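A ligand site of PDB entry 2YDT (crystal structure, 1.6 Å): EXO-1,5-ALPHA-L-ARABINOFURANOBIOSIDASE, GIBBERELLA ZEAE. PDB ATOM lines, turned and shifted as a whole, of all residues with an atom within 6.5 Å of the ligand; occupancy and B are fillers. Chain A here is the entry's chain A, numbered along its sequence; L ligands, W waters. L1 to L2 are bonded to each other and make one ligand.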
ATOM      1  N   PRO A  26      28.751   8.678 -30.411  1.00  0.00           N
ATOM      2  CA  PRO A  26      29.773   8.616 -31.479  1.00  0.00           C
ATOM      3  C   PRO A  26      31.124   8.021 -31.074  1.00  0.00           C
ATOM      4  O   PRO A  26      32.048   8.017 -31.900  1.00  0.00           O
ATOM      5  CB  PRO A  26      29.942  10.087 -31.852  1.00  0.00           C
ATOM      6  CG  PRO A  26      29.816  10.778 -30.537  1.00  0.00           C
ATOM      7  CD  PRO A  26      28.709  10.042 -29.822  1.00  0.00           C
ATOM      8  N   LEU A  29      34.688  12.128 -29.660  1.00  0.00           N
ATOM      9  CA  LEU A  29      34.294  13.378 -30.309  1.00  0.00           C
ATOM     10  C   LEU A  29      35.098  14.465 -29.591  1.00  0.00           C
ATOM     11  O   LEU A  29      35.551  14.283 -28.454  1.00  0.00           O
ATOM     12  CB  LEU A  29      32.784  13.627 -30.126  1.00  0.00           C
ATOM     13  CG  LEU A  29      32.139  14.652 -31.058  1.00  0.00           C
ATOM     14  CD1 LEU A  29      32.057  14.106 -32.519  1.00  0.00           C
ATOM     15  CD2 LEU A  29      30.769  15.115 -30.539  1.00  0.00           C
ATOM     16  N   TYR A  30      35.269  15.632 -30.231  1.00  0.00           N
ATOM     17  CA  TYR A  30      35.705  16.836 -29.481  1.00  0.00           C
ATOM     18  C   TYR A  30      37.140  16.750 -29.015  1.00  0.00           C
ATOM     19  O   TYR A  30      37.431  16.816 -27.820  1.00  0.00           O
ATOM     20  CB  TYR A  30      34.728  17.137 -28.316  1.00  0.00           C
ATOM     21  CG  TYR A  30      34.558  18.619 -28.014  1.00  0.00           C
ATOM     22  CD1 TYR A  30      33.374  19.292 -28.361  1.00  0.00           C
ATOM     23  CD2 TYR A  30      35.533  19.330 -27.336  1.00  0.00           C
ATOM     24  CE1 TYR A  30      33.181  20.610 -28.092  1.00  0.00           C
ATOM     25  CE2 TYR A  30      35.365  20.676 -27.043  1.00  0.00           C
ATOM     26  CZ  TYR A  30      34.181  21.307 -27.402  1.00  0.00           C
ATOM     27  OH  TYR A  30      33.991  22.658 -27.126  1.00  0.00           O
ATOM     28  N   GLU A  46      36.081  13.757 -25.727  1.00  0.00           N
ATOM     29  CA  GLU A  46      34.887  13.132 -25.111  1.00  0.00           C
ATOM     30  C   GLU A  46      34.977  11.640 -25.351  1.00  0.00           C
ATOM     31  O   GLU A  46      35.071  11.205 -26.492  1.00  0.00           O
ATOM     32  CB  GLU A  46      33.592  13.635 -25.738  1.00  0.00           C
ATOM     33  CG  GLU A  46      33.341  15.116 -25.566  1.00  0.00           C
ATOM     34  CD  GLU A  46      32.150  15.661 -26.356  1.00  0.00           C
ATOM     35  OE1 GLU A  46      31.555  14.957 -27.170  1.00  0.00           O
ATOM     36  OE2 GLU A  46      31.846  16.846 -26.149  1.00  0.00           O
ATOM     37  N   TYR A  48      33.123   8.129 -24.867  1.00  0.00           N
ATOM     38  CA  TYR A  48      31.748   7.635 -24.663  1.00  0.00           C
ATOM     39  C   TYR A  48      31.775   6.162 -24.246  1.00  0.00           C
ATOM     40  O   TYR A  48      31.199   5.281 -24.898  1.00  0.00           O
ATOM     41  CB  TYR A  48      30.865   7.855 -25.898  1.00  0.00           C
ATOM     42  CG  TYR A  48      30.538   9.288 -26.230  1.00  0.00           C
ATOM     43  CD1 TYR A  48      29.275   9.792 -26.014  1.00  0.00           C
ATOM     44  CD2 TYR A  48      31.499  10.157 -26.769  1.00  0.00           C
ATOM     45  CE1 TYR A  48      28.940  11.129 -26.308  1.00  0.00           C
ATOM     46  CE2 TYR A  48      31.187  11.480 -27.051  1.00  0.00           C
ATOM     47  CZ  TYR A  48      29.908  11.966 -26.832  1.00  0.00           C
ATOM     48  OH  TYR A  48      29.578  13.279 -27.105  1.00  0.00           O
ATOM     49  N   ARG A  85      31.743  14.605 -19.131  1.00  0.00           N
ATOM     50  CA  ARG A  85      31.059  14.028 -20.291  1.00  0.00           C
ATOM     51  C   ARG A  85      31.315  14.782 -21.596  1.00  0.00           C
ATOM     52  O   ARG A  85      31.647  14.161 -22.607  1.00  0.00           O
ATOM     53  CB  ARG A  85      29.563  13.910 -20.008  1.00  0.00           C
ATOM     54  CG  ARG A  85      28.795  13.077 -21.072  1.00  0.00           C
ATOM     55  CD  ARG A  85      27.342  12.859 -20.665  1.00  0.00           C
ATOM     56  NE  ARG A  85      27.267  12.256 -19.320  1.00  0.00           N
ATOM     57  CZ  ARG A  85      27.457  10.965 -19.040  1.00  0.00           C
ATOM     58  NH1 ARG A  85      27.630  10.062 -19.985  1.00  0.00           N
ATOM     59  NH2 ARG A  85      27.429  10.554 -17.777  1.00  0.00           N
ATOM     60  N   TYR A  86      31.095  16.097 -21.591  1.00  0.00           N
ATOM     61  CA  TYR A  86      31.130  16.868 -22.835  1.00  0.00           C
ATOM     62  C   TYR A  86      32.190  17.984 -22.794  1.00  0.00           C
ATOM     63  O   TYR A  86      32.430  18.574 -21.756  1.00  0.00           O
ATOM     64  CB  TYR A  86      29.778  17.552 -23.131  1.00  0.00           C
ATOM     65  CG  TYR A  86      28.651  16.694 -23.666  1.00  0.00           C
ATOM     66  CD1 TYR A  86      28.844  15.379 -24.118  1.00  0.00           C
ATOM     67  CD2 TYR A  86      27.380  17.246 -23.769  1.00  0.00           C
ATOM     68  CE1 TYR A  86      27.795  14.627 -24.660  1.00  0.00           C
ATOM     69  CE2 TYR A  86      26.328  16.502 -24.306  1.00  0.00           C
ATOM     70  CZ  TYR A  86      26.541  15.191 -24.736  1.00  0.00           C
ATOM     71  OH  TYR A  86      25.492  14.481 -25.288  1.00  0.00           O
ATOM     72  N   GLN A  87      32.762  18.264 -23.957  1.00  0.00           N
ATOM     73  CA  GLN A  87      33.438  19.541 -24.239  1.00  0.00           C
ATOM     74  C   GLN A  87      34.634  19.877 -23.363  1.00  0.00           C
ATOM     75  O   GLN A  87      34.747  20.984 -22.859  1.00  0.00           O
ATOM     76  CB  GLN A  87      32.381  20.658 -24.243  1.00  0.00           C
ATOM     77  CG  GLN A  87      31.278  20.411 -25.289  1.00  0.00           C
ATOM     78  CD  GLN A  87      29.849  20.610 -24.810  1.00  0.00           C
ATOM     79  OE1 GLN A  87      29.602  21.260 -23.792  1.00  0.00           O
ATOM     80  NE2 GLN A  87      28.903  20.038 -25.550  1.00  0.00           N
ATOM     81  N   ALA A 145      21.006  18.789 -21.248  1.00  0.00           N
ATOM     82  CA  ALA A 145      22.036  18.820 -22.288  1.00  0.00           C
ATOM     83  C   ALA A 145      21.567  18.387 -23.658  1.00  0.00           C
ATOM     84  O   ALA A 145      22.158  17.481 -24.252  1.00  0.00           O
ATOM     85  CB  ALA A 145      23.258  17.941 -21.820  1.00  0.00           C
ATOM     86  N   LEU A 146      20.554  19.081 -24.189  1.00  0.00           N
ATOM     87  CA  LEU A 146      20.156  18.957 -25.589  1.00  0.00           C
ATOM     88  C   LEU A 146      20.089  20.345 -26.177  1.00  0.00           C
ATOM     89  O   LEU A 146      19.656  21.274 -25.498  1.00  0.00           O
ATOM     90  CB  LEU A 146      18.777  18.277 -25.711  1.00  0.00           C
ATOM     91  CG  LEU A 146      18.653  16.872 -25.190  1.00  0.00           C
ATOM     92  CD1 LEU A 146      17.156  16.468 -25.244  1.00  0.00           C
ATOM     93  CD2 LEU A 146      19.507  15.952 -26.010  1.00  0.00           C
ATOM     94  N   PRO A 147      20.543  20.521 -27.432  1.00  0.00           N
ATOM     95  CA  PRO A 147      20.637  21.878 -28.023  1.00  0.00           C
ATOM     96  C   PRO A 147      19.316  22.360 -28.623  1.00  0.00           C
ATOM     97  O   PRO A 147      19.230  22.644 -29.841  1.00  0.00           O
ATOM     98  CB  PRO A 147      21.697  21.704 -29.125  1.00  0.00           C
ATOM     99  CG  PRO A 147      21.472  20.288 -29.559  1.00  0.00           C
ATOM    100  CD  PRO A 147      21.201  19.515 -28.287  1.00  0.00           C
ATOM    101  N   ASN A 148      18.285  22.380 -27.787  1.00  0.00           N
ATOM    102  CA  ASN A 148      16.906  22.663 -28.181  1.00  0.00           C
ATOM    103  C   ASN A 148      16.445  23.972 -27.571  1.00  0.00           C
ATOM    104  O   ASN A 148      16.737  24.253 -26.415  1.00  0.00           O
ATOM    105  CB  ASN A 148      15.994  21.550 -27.672  1.00  0.00           C
ATOM    106  CG  ASN A 148      16.254  20.178 -28.339  1.00  0.00           C
ATOM    107  OD1 ASN A 148      16.934  20.087 -29.357  1.00  0.00           O
ATOM    108  ND2 ASN A 148      15.623  19.134 -27.791  1.00  0.00           N
ATOM    109  N   PRO A 153      20.652  24.550 -20.955  1.00  0.00           N
ATOM    110  CA  PRO A 153      22.026  24.119 -20.714  1.00  0.00           C
ATOM    111  C   PRO A 153      23.117  25.164 -20.937  1.00  0.00           C
ATOM    112  O   PRO A 153      22.904  26.173 -21.608  1.00  0.00           O
ATOM    113  CB  PRO A 153      22.220  22.956 -21.694  1.00  0.00           C
ATOM    114  CG  PRO A 153      21.303  23.313 -22.834  1.00  0.00           C
ATOM    115  CD  PRO A 153      20.093  23.923 -22.159  1.00  0.00           C
ATOM    116  N   TRP A 155      27.411  25.097 -22.177  1.00  0.00           N
ATOM    117  CA  TRP A 155      28.279  24.244 -22.984  1.00  0.00           C
ATOM    118  C   TRP A 155      29.608  24.896 -23.311  1.00  0.00           C
ATOM    119  O   TRP A 155      29.740  26.115 -23.360  1.00  0.00           O
ATOM    120  CB  TRP A 155      27.685  23.947 -24.354  1.00  0.00           C
ATOM    121  CG  TRP A 155      26.176  23.770 -24.531  1.00  0.00           C
ATOM    122  CD1 TRP A 155      25.253  24.773 -24.826  1.00  0.00           C
ATOM    123  CD2 TRP A 155      25.471  22.546 -24.645  1.00  0.00           C
ATOM    124  NE1 TRP A 155      24.030  24.216 -25.049  1.00  0.00           N
ATOM    125  CE2 TRP A 155      24.127  22.852 -24.984  1.00  0.00           C
ATOM    126  CE3 TRP A 155      25.829  21.205 -24.472  1.00  0.00           C
ATOM    127  CZ2 TRP A 155      23.167  21.842 -25.221  1.00  0.00           C
ATOM    128  CZ3 TRP A 155      24.884  20.218 -24.663  1.00  0.00           C
ATOM    129  CH2 TRP A 155      23.559  20.531 -25.024  1.00  0.00           C
ATOM    130  N   GLU A 156      30.571  24.056 -23.646  1.00  0.00           N
ATOM    131  CA  GLU A 156      31.708  24.456 -24.523  1.00  0.00           C
ATOM    132  C   GLU A 156      32.654  25.513 -23.956  1.00  0.00           C
ATOM    133  O   GLU A 156      32.858  26.583 -24.598  1.00  0.00           O
ATOM    134  CB  GLU A 156      31.178  24.886 -25.925  1.00  0.00           C
ATOM    135  CG  GLU A 156      30.522  23.698 -26.673  1.00  0.00           C
ATOM    136  CD  GLU A 156      29.321  24.031 -27.572  1.00  0.00           C
ATOM    137  OE1 GLU A 156      28.854  25.177 -27.622  1.00  0.00           O
ATOM    138  OE2 GLU A 156      28.857  23.068 -28.238  1.00  0.00           O
ATOM    139  N   SER A 171      28.971  28.819 -24.080  1.00  0.00           N
ATOM    140  CA  SER A 171      27.647  28.879 -24.714  1.00  0.00           C
ATOM    141  C   SER A 171      26.564  28.723 -23.646  1.00  0.00           C
ATOM    142  O   SER A 171      26.681  27.848 -22.782  1.00  0.00           O
ATOM    143  CB  SER A 171      27.492  27.761 -25.751  1.00  0.00           C
ATOM    144  OG  SER A 171      28.579  27.766 -26.685  1.00  0.00           O
ATOM    145  N   GLN A 173      22.323  28.753 -22.700  1.00  0.00           N
ATOM    146  CA  GLN A 173      20.901  28.738 -23.051  1.00  0.00           C
ATOM    147  C   GLN A 173      20.002  29.187 -21.904  1.00  0.00           C
ATOM    148  O   GLN A 173      18.794  29.083 -22.021  1.00  0.00           O
ATOM    149  CB  GLN A 173      20.429  27.326 -23.511  1.00  0.00           C
ATOM    150  CG  GLN A 173      21.088  26.857 -24.801  1.00  0.00           C
ATOM    151  CD  GLN A 173      20.482  25.625 -25.476  1.00  0.00           C
ATOM    152  OE1 GLN A 173      21.245  24.817 -26.023  1.00  0.00           O
ATOM    153  NE2 GLN A 173      19.129  25.482 -25.469  1.00  0.00           N
ATOM    154  N   GLN A 181      20.064  30.470 -27.785  1.00  0.00           N
ATOM    155  CA  GLN A 181      21.371  30.393 -27.148  1.00  0.00           C
ATOM    156  C   GLN A 181      22.057  31.752 -27.325  1.00  0.00           C
ATOM    157  O   GLN A 181      21.804  32.470 -28.320  1.00  0.00           O
ATOM    158  CB  GLN A 181      22.245  29.291 -27.738  1.00  0.00           C
ATOM    159  CG  GLN A 181      23.495  28.971 -26.919  1.00  0.00           C
ATOM    160  CD  GLN A 181      24.241  27.755 -27.431  1.00  0.00           C
ATOM    161  OE1 GLN A 181      23.996  26.648 -26.979  1.00  0.00           O
ATOM    162  NE2 GLN A 181      25.091  27.941 -28.464  1.00  0.00           N
ATOM    163  N   LEU A 183      26.186  33.707 -26.170  1.00  0.00           N
ATOM    164  CA  LEU A 183      27.583  33.482 -25.826  1.00  0.00           C
ATOM    165  C   LEU A 183      27.953  34.428 -24.694  1.00  0.00           C
ATOM    166  O   LEU A 183      27.599  35.618 -24.733  1.00  0.00           O
ATOM    167  CB  LEU A 183      28.493  33.723 -27.043  1.00  0.00           C
ATOM    168  CG  LEU A 183      28.322  32.673 -28.121  1.00  0.00           C
ATOM    169  CD1 LEU A 183      29.035  33.054 -29.395  1.00  0.00           C
ATOM    170  CD2 LEU A 183      28.849  31.298 -27.607  1.00  0.00           C
ATOM    171  N   ARG A 209      21.294  31.034 -32.694  1.00  0.00           N
ATOM    172  CA  ARG A 209      22.089  30.202 -31.764  1.00  0.00           C
ATOM    173  C   ARG A 209      23.566  30.400 -32.068  1.00  0.00           C
ATOM    174  O   ARG A 209      24.259  29.497 -32.568  1.00  0.00           O
ATOM    175  CB  ARG A 209      21.699  28.730 -31.815  1.00  0.00           C
ATOM    176  CG  ARG A 209      20.300  28.455 -31.310  1.00  0.00           C
ATOM    177  CD  ARG A 209      19.907  27.006 -31.579  1.00  0.00           C
ATOM    178  NE  ARG A 209      20.739  26.110 -30.806  1.00  0.00           N
ATOM    179  CZ  ARG A 209      20.626  25.884 -29.507  1.00  0.00           C
ATOM    180  NH1 ARG A 209      19.604  26.347 -28.789  1.00  0.00           N
ATOM    181  NH2 ARG A 209      21.521  25.118 -28.923  1.00  0.00           N
ATOM    182  N   PRO A 210      24.124  31.588 -31.737  1.00  0.00           N
ATOM    183  CA  PRO A 210      25.585  31.709 -31.724  1.00  0.00           C
ATOM    184  C   PRO A 210      26.146  30.732 -30.708  1.00  0.00           C
ATOM    185  O   PRO A 210      25.546  30.576 -29.643  1.00  0.00           O
ATOM    186  CB  PRO A 210      25.820  33.169 -31.300  1.00  0.00           C
ATOM    187  CG  PRO A 210      24.607  33.481 -30.448  1.00  0.00           C
ATOM    188  CD  PRO A 210      23.466  32.772 -31.138  1.00  0.00           C
ATOM    189  N   GLY A 211      27.230  30.080 -31.067  1.00  0.00           N
ATOM    190  CA  GLY A 211      27.786  29.004 -30.246  1.00  0.00           C
ATOM    191  C   GLY A 211      29.260  28.738 -30.515  1.00  0.00           C
ATOM    192  O   GLY A 211      29.843  29.140 -31.540  1.00  0.00           O
ATOM    193  N   MET A 212      29.877  28.047 -29.574  1.00  0.00           N
ATOM    194  CA  MET A 212      31.214  27.405 -29.751  1.00  0.00           C
ATOM    195  C   MET A 212      32.362  28.459 -29.848  1.00  0.00           C
ATOM    196  O   MET A 212      33.048  28.602 -30.896  1.00  0.00           O
ATOM    197  CB  MET A 212      31.198  26.437 -30.940  1.00  0.00           C
ATOM    198  CG  MET A 212      29.985  25.528 -30.913  1.00  0.00           C
ATOM    199  SD  MET A 212      30.063  24.074 -31.952  1.00  0.00           S
ATOM    200  CE  MET A 212      31.236  23.080 -30.977  1.00  0.00           C
ATOM    201  N   PRO A 213      32.591  29.223 -28.767  1.00  0.00           N
ATOM    202  CA  PRO A 213      33.536  30.355 -28.818  1.00  0.00           C
ATOM    203  C   PRO A 213      34.996  29.915 -28.686  1.00  0.00           C
ATOM    204  O   PRO A 213      35.322  29.112 -27.796  1.00  0.00           O
ATOM    205  CB  PRO A 213      33.122  31.226 -27.641  1.00  0.00           C
ATOM    206  CG  PRO A 213      32.671  30.183 -26.628  1.00  0.00           C
ATOM    207  CD  PRO A 213      31.935  29.120 -27.457  1.00  0.00           C
ATOM    208  N   GLU A 228      30.368  29.899 -34.267  1.00  0.00           N
ATOM    209  CA  GLU A 228      29.348  29.561 -35.305  1.00  0.00           C
ATOM    210  C   GLU A 228      28.085  30.369 -35.020  1.00  0.00           C
ATOM    211  O   GLU A 228      27.573  30.401 -33.894  1.00  0.00           O
ATOM    212  CB  GLU A 228      29.090  28.057 -35.369  1.00  0.00           C
ATOM    213  CG  GLU A 228      28.377  27.458 -34.150  1.00  0.00           C
ATOM    214  CD  GLU A 228      27.940  25.976 -34.340  1.00  0.00           C
ATOM    215  OE1 GLU A 228      28.444  25.318 -35.302  1.00  0.00           O
ATOM    216  OE2 GLU A 228      27.104  25.479 -33.557  1.00  0.00           O
ATOM    217  N   PHE A 243      24.968  27.466 -39.870  1.00  0.00           N
ATOM    218  CA  PHE A 243      25.903  27.856 -38.815  1.00  0.00           C
ATOM    219  C   PHE A 243      27.197  28.448 -39.392  1.00  0.00           C
ATOM    220  O   PHE A 243      28.307  28.001 -39.093  1.00  0.00           O
ATOM    221  CB  PHE A 243      26.212  26.607 -37.945  1.00  0.00           C
ATOM    222  CG  PHE A 243      25.009  26.014 -37.229  1.00  0.00           C
ATOM    223  CD1 PHE A 243      24.714  26.337 -35.906  1.00  0.00           C
ATOM    224  CD2 PHE A 243      24.157  25.128 -37.884  1.00  0.00           C
ATOM    225  CE1 PHE A 243      23.591  25.800 -35.272  1.00  0.00           C
ATOM    226  CE2 PHE A 243      23.065  24.593 -37.241  1.00  0.00           C
ATOM    227  CZ  PHE A 243      22.791  24.914 -35.945  1.00  0.00           C
ATOM    228  N   TYR A 323      34.054  17.376 -36.521  1.00  0.00           N
ATOM    229  CA  TYR A 323      33.367  18.283 -35.614  1.00  0.00           C
ATOM    230  C   TYR A 323      34.341  18.901 -34.641  1.00  0.00           C
ATOM    231  O   TYR A 323      35.158  18.204 -34.007  1.00  0.00           O
ATOM    232  CB  TYR A 323      32.285  17.527 -34.855  1.00  0.00           C
ATOM    233  CG  TYR A 323      31.442  18.354 -33.917  1.00  0.00           C
ATOM    234  CD1 TYR A 323      30.525  19.293 -34.400  1.00  0.00           C
ATOM    235  CD2 TYR A 323      31.522  18.176 -32.521  1.00  0.00           C
ATOM    236  CE1 TYR A 323      29.739  20.055 -33.528  1.00  0.00           C
ATOM    237  CE2 TYR A 323      30.738  18.930 -31.655  1.00  0.00           C
ATOM    238  CZ  TYR A 323      29.834  19.856 -32.170  1.00  0.00           C
ATOM    239  OH  TYR A 323      29.032  20.556 -31.321  1.00  0.00           O
ATOM    240  N   LEU A 345      29.807  14.148 -35.712  1.00  0.00           N
ATOM    241  CA  LEU A 345      28.642  14.042 -34.861  1.00  0.00           C
ATOM    242  C   LEU A 345      27.908  12.725 -35.070  1.00  0.00           C
ATOM    243  O   LEU A 345      27.948  12.171 -36.192  1.00  0.00           O
ATOM    244  CB  LEU A 345      27.672  15.196 -35.168  1.00  0.00           C
ATOM    245  CG  LEU A 345      28.136  16.551 -34.636  1.00  0.00           C
ATOM    246  CD1 LEU A 345      27.323  17.667 -35.390  1.00  0.00           C
ATOM    247  CD2 LEU A 345      27.925  16.639 -33.145  1.00  0.00           C
ATOM    248  N   PRO A 346      27.248  12.215 -34.016  1.00  0.00           N
ATOM    249  CA  PRO A 346      26.464  10.980 -34.242  1.00  0.00           C
ATOM    250  C   PRO A 346      25.302  11.240 -35.221  1.00  0.00           C
ATOM    251  O   PRO A 346      24.733  12.341 -35.261  1.00  0.00           O
ATOM    252  CB  PRO A 346      25.983  10.612 -32.838  1.00  0.00           C
ATOM    253  CG  PRO A 346      25.924  11.910 -32.146  1.00  0.00           C
ATOM    254  CD  PRO A 346      27.057  12.703 -32.646  1.00  0.00           C
HETATM  255  O1  LIG L   1      26.908  25.867 -29.276  1.00  0.00           O
HETATM  256  C1  LIG L   1      25.975  24.836 -29.703  1.00  0.00           C
HETATM  257  C2  LIG L   1      26.648  23.947 -30.726  1.00  0.00           C
HETATM  258  N1  LIG L   1      26.768  22.635 -30.066  1.00  0.00           N
HETATM  259  C3  LIG L   1      25.511  23.929 -28.564  1.00  0.00           C
HETATM  260  O2  LIG L   1      24.136  24.158 -28.155  1.00  0.00           O
HETATM  261  C4  LIG L   1      25.658  22.510 -29.140  1.00  0.00           C
HETATM  262  C5  LIG L   1      25.846  21.416 -28.120  1.00  0.00           C
HETATM  263  O3  LIG L   1      25.695  20.178 -28.798  1.00  0.00           O
HETATM  264  O1  LG2 L   2      29.882  17.945 -27.498  1.00  0.00           O
HETATM  265  C1  LG2 L   2      28.772  17.043 -27.677  1.00  0.00           C
HETATM  266  C2  LG2 L   2      27.612  17.717 -28.374  1.00  0.00           C
HETATM  267  O2  LG2 L   2      27.073  18.785 -27.613  1.00  0.00           O
HETATM  268  C3  LG2 L   2      26.394  16.793 -28.541  1.00  0.00           C
HETATM  269  O3  LG2 L   2      26.519  15.882 -29.669  1.00  0.00           O
HETATM  270  C4  LG2 L   2      25.295  17.793 -28.803  1.00  0.00           C
HETATM  271  O4  LG2 L   2      23.973  17.374 -28.425  1.00  0.00           O
HETATM  272  C5  LG2 L   2      25.734  18.986 -28.013  1.00  0.00           C
HETATM  273  O   HOH W   1      25.174  26.838 -32.200  1.00  0.00           O
HETATM  274  O   HOH W   2      22.583  17.088 -30.708  1.00  0.00           O
HETATM  275  O   HOH W   3      24.410  15.089 -31.225  1.00  0.00           O
HETATM  276  O   HOH W   4      27.499  13.456 -28.990  1.00  0.00           O
HETATM  277  O   HOH W   5      26.211  20.915 -32.186  1.00  0.00           O
HETATM  278  O   HOH W   6      23.396  15.900 -26.193  1.00  0.00           O
HETATM  279  O   HOH W   7      29.906  20.536 -28.799  1.00  0.00           O
HETATM  280  O   HOH W   8      23.107  25.006 -31.678  1.00  0.00           O
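An oxygen (O1) of LG2 L2 sits at hydrogen-bond distance from the side-chain carboxylate of Glu 46 (2.6 Å).
The side-chain carboxylate (OE2) of Glu 156 is in salt-bridge range of a nitrogen (N1) of LIG L1, 2.8 Å away.
The side-chain amide oxygen (OE1) of Gln 181 sits at hydrogen-bond distance from an oxygen (O2) of LIG L1 (2.8 Å).
O2 of LIG L1 is in hydrogen-bond range of NH2 of Arg 209 (2.9 Å).
NE2 of Gln 87 is in hydrogen-bond range of O1 of LG2 L2 (3.0 Å).
An oxygen (O2) of LIG L1 is in hydrogen-bond range of the indole nitrogen (NE1) of Trp 155 (3.1 Å).
The side-chain hydroxyl (OH) of Tyr 323 is in hydrogen-bond range of a nitrogen (N1) of LIG L1 (3.3 Å).
OE2 of Glu 46 is in hydrogen-bond range of N of Gln 87 (2.8 Å).
O of Leu 29 is in hydrogen-bond range of N of Glu 46 (2.8 Å).
OE1 of Gln 181 sits at hydrogen-bond distance from NH2 of Arg 209, at 3.5 Å.
The side-chain amide nitrogen of Gln 181 lies within hydrogen-bond range of the backbone carbonyl oxygen of Pro 210 (2.9 Å).
The guanidinium group (NH2) of Arg 209 lies close to the backbone carbonyl oxygen (O) of Pro 147.
The side-chain amide oxygen (OE1) of Gln 173 sits at hydrogen-bond distance from the guanidinium group (NH2) of Arg 209, at 2.9 Å.
The side-chain amide oxygen (OE1) of Gln 173 lies within hydrogen-bond range of the indole nitrogen (NE1) of Trp 155.
The backbone NH (N) of Gly 211 lies within hydrogen-bond range of the backbone carbonyl oxygen (O) of Glu 228, at 2.9 Å.
CD2 of Leu 29 touches C1 of LG2 L2 (3.99 Å).
CD1 of Tyr 30 touches O1 of LG2 L2 (3.8 Å).
OH of Tyr 48 touches C1 of LG2 L2, 3.9 Å away.
Tyr 86 touches the ligand.
CD of Pro 147 touches O4 of LG2 L2 (3.5 Å).
OG of Ser 171 touches O1 of LIG L1 (3.6 Å).
OE1 of Gln 173 touches O2 of LIG L1 (3.7 Å).
CA of Gly 211 touches O1 of LIG L1, 3.4 Å away.
Met 212 touches the ligand.
OE2 of Glu 228 touches C2 of LIG L1, at 3.3 Å.
CD2 of Leu 345 touches O3 of LG2 L2 (3.8 Å).
Hydrophobic or aromatic side chains within 4 Å of the ligand: Leu 29, Tyr 30, Tyr 86, Pro 147, Trp 155, Met 212 and Leu 345.
The nearest printed residue that does not touch the ligand is Pro 346 (4.4 Å).
Water W4 bridges O3 of LG2 L2 (2.7 Å) and OH of Tyr 48 (2.8 Å).
Water W6 lies within hydrogen-bond range of OH of Tyr 86, O4 of LG2 L2 and O of Ala 145.
Water W5 lies within hydrogen-bond range of a nitrogen (N1) of LIG L1 (2.8 Å) and the side-chain hydroxyl of Tyr 323 (3.0 Å).
Water W7 lies within hydrogen-bond range of OH of Tyr 323 (2.7 Å), OE2 of Glu 156 (2.8 Å), O1 of LG2 L2 (2.9 Å) and NE2 of Gln 87 (3.4 Å).
Water W1 lies within hydrogen-bond range of OE2 of Glu 228 (2.7 Å) and O of Arg 209 (2.8 Å).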
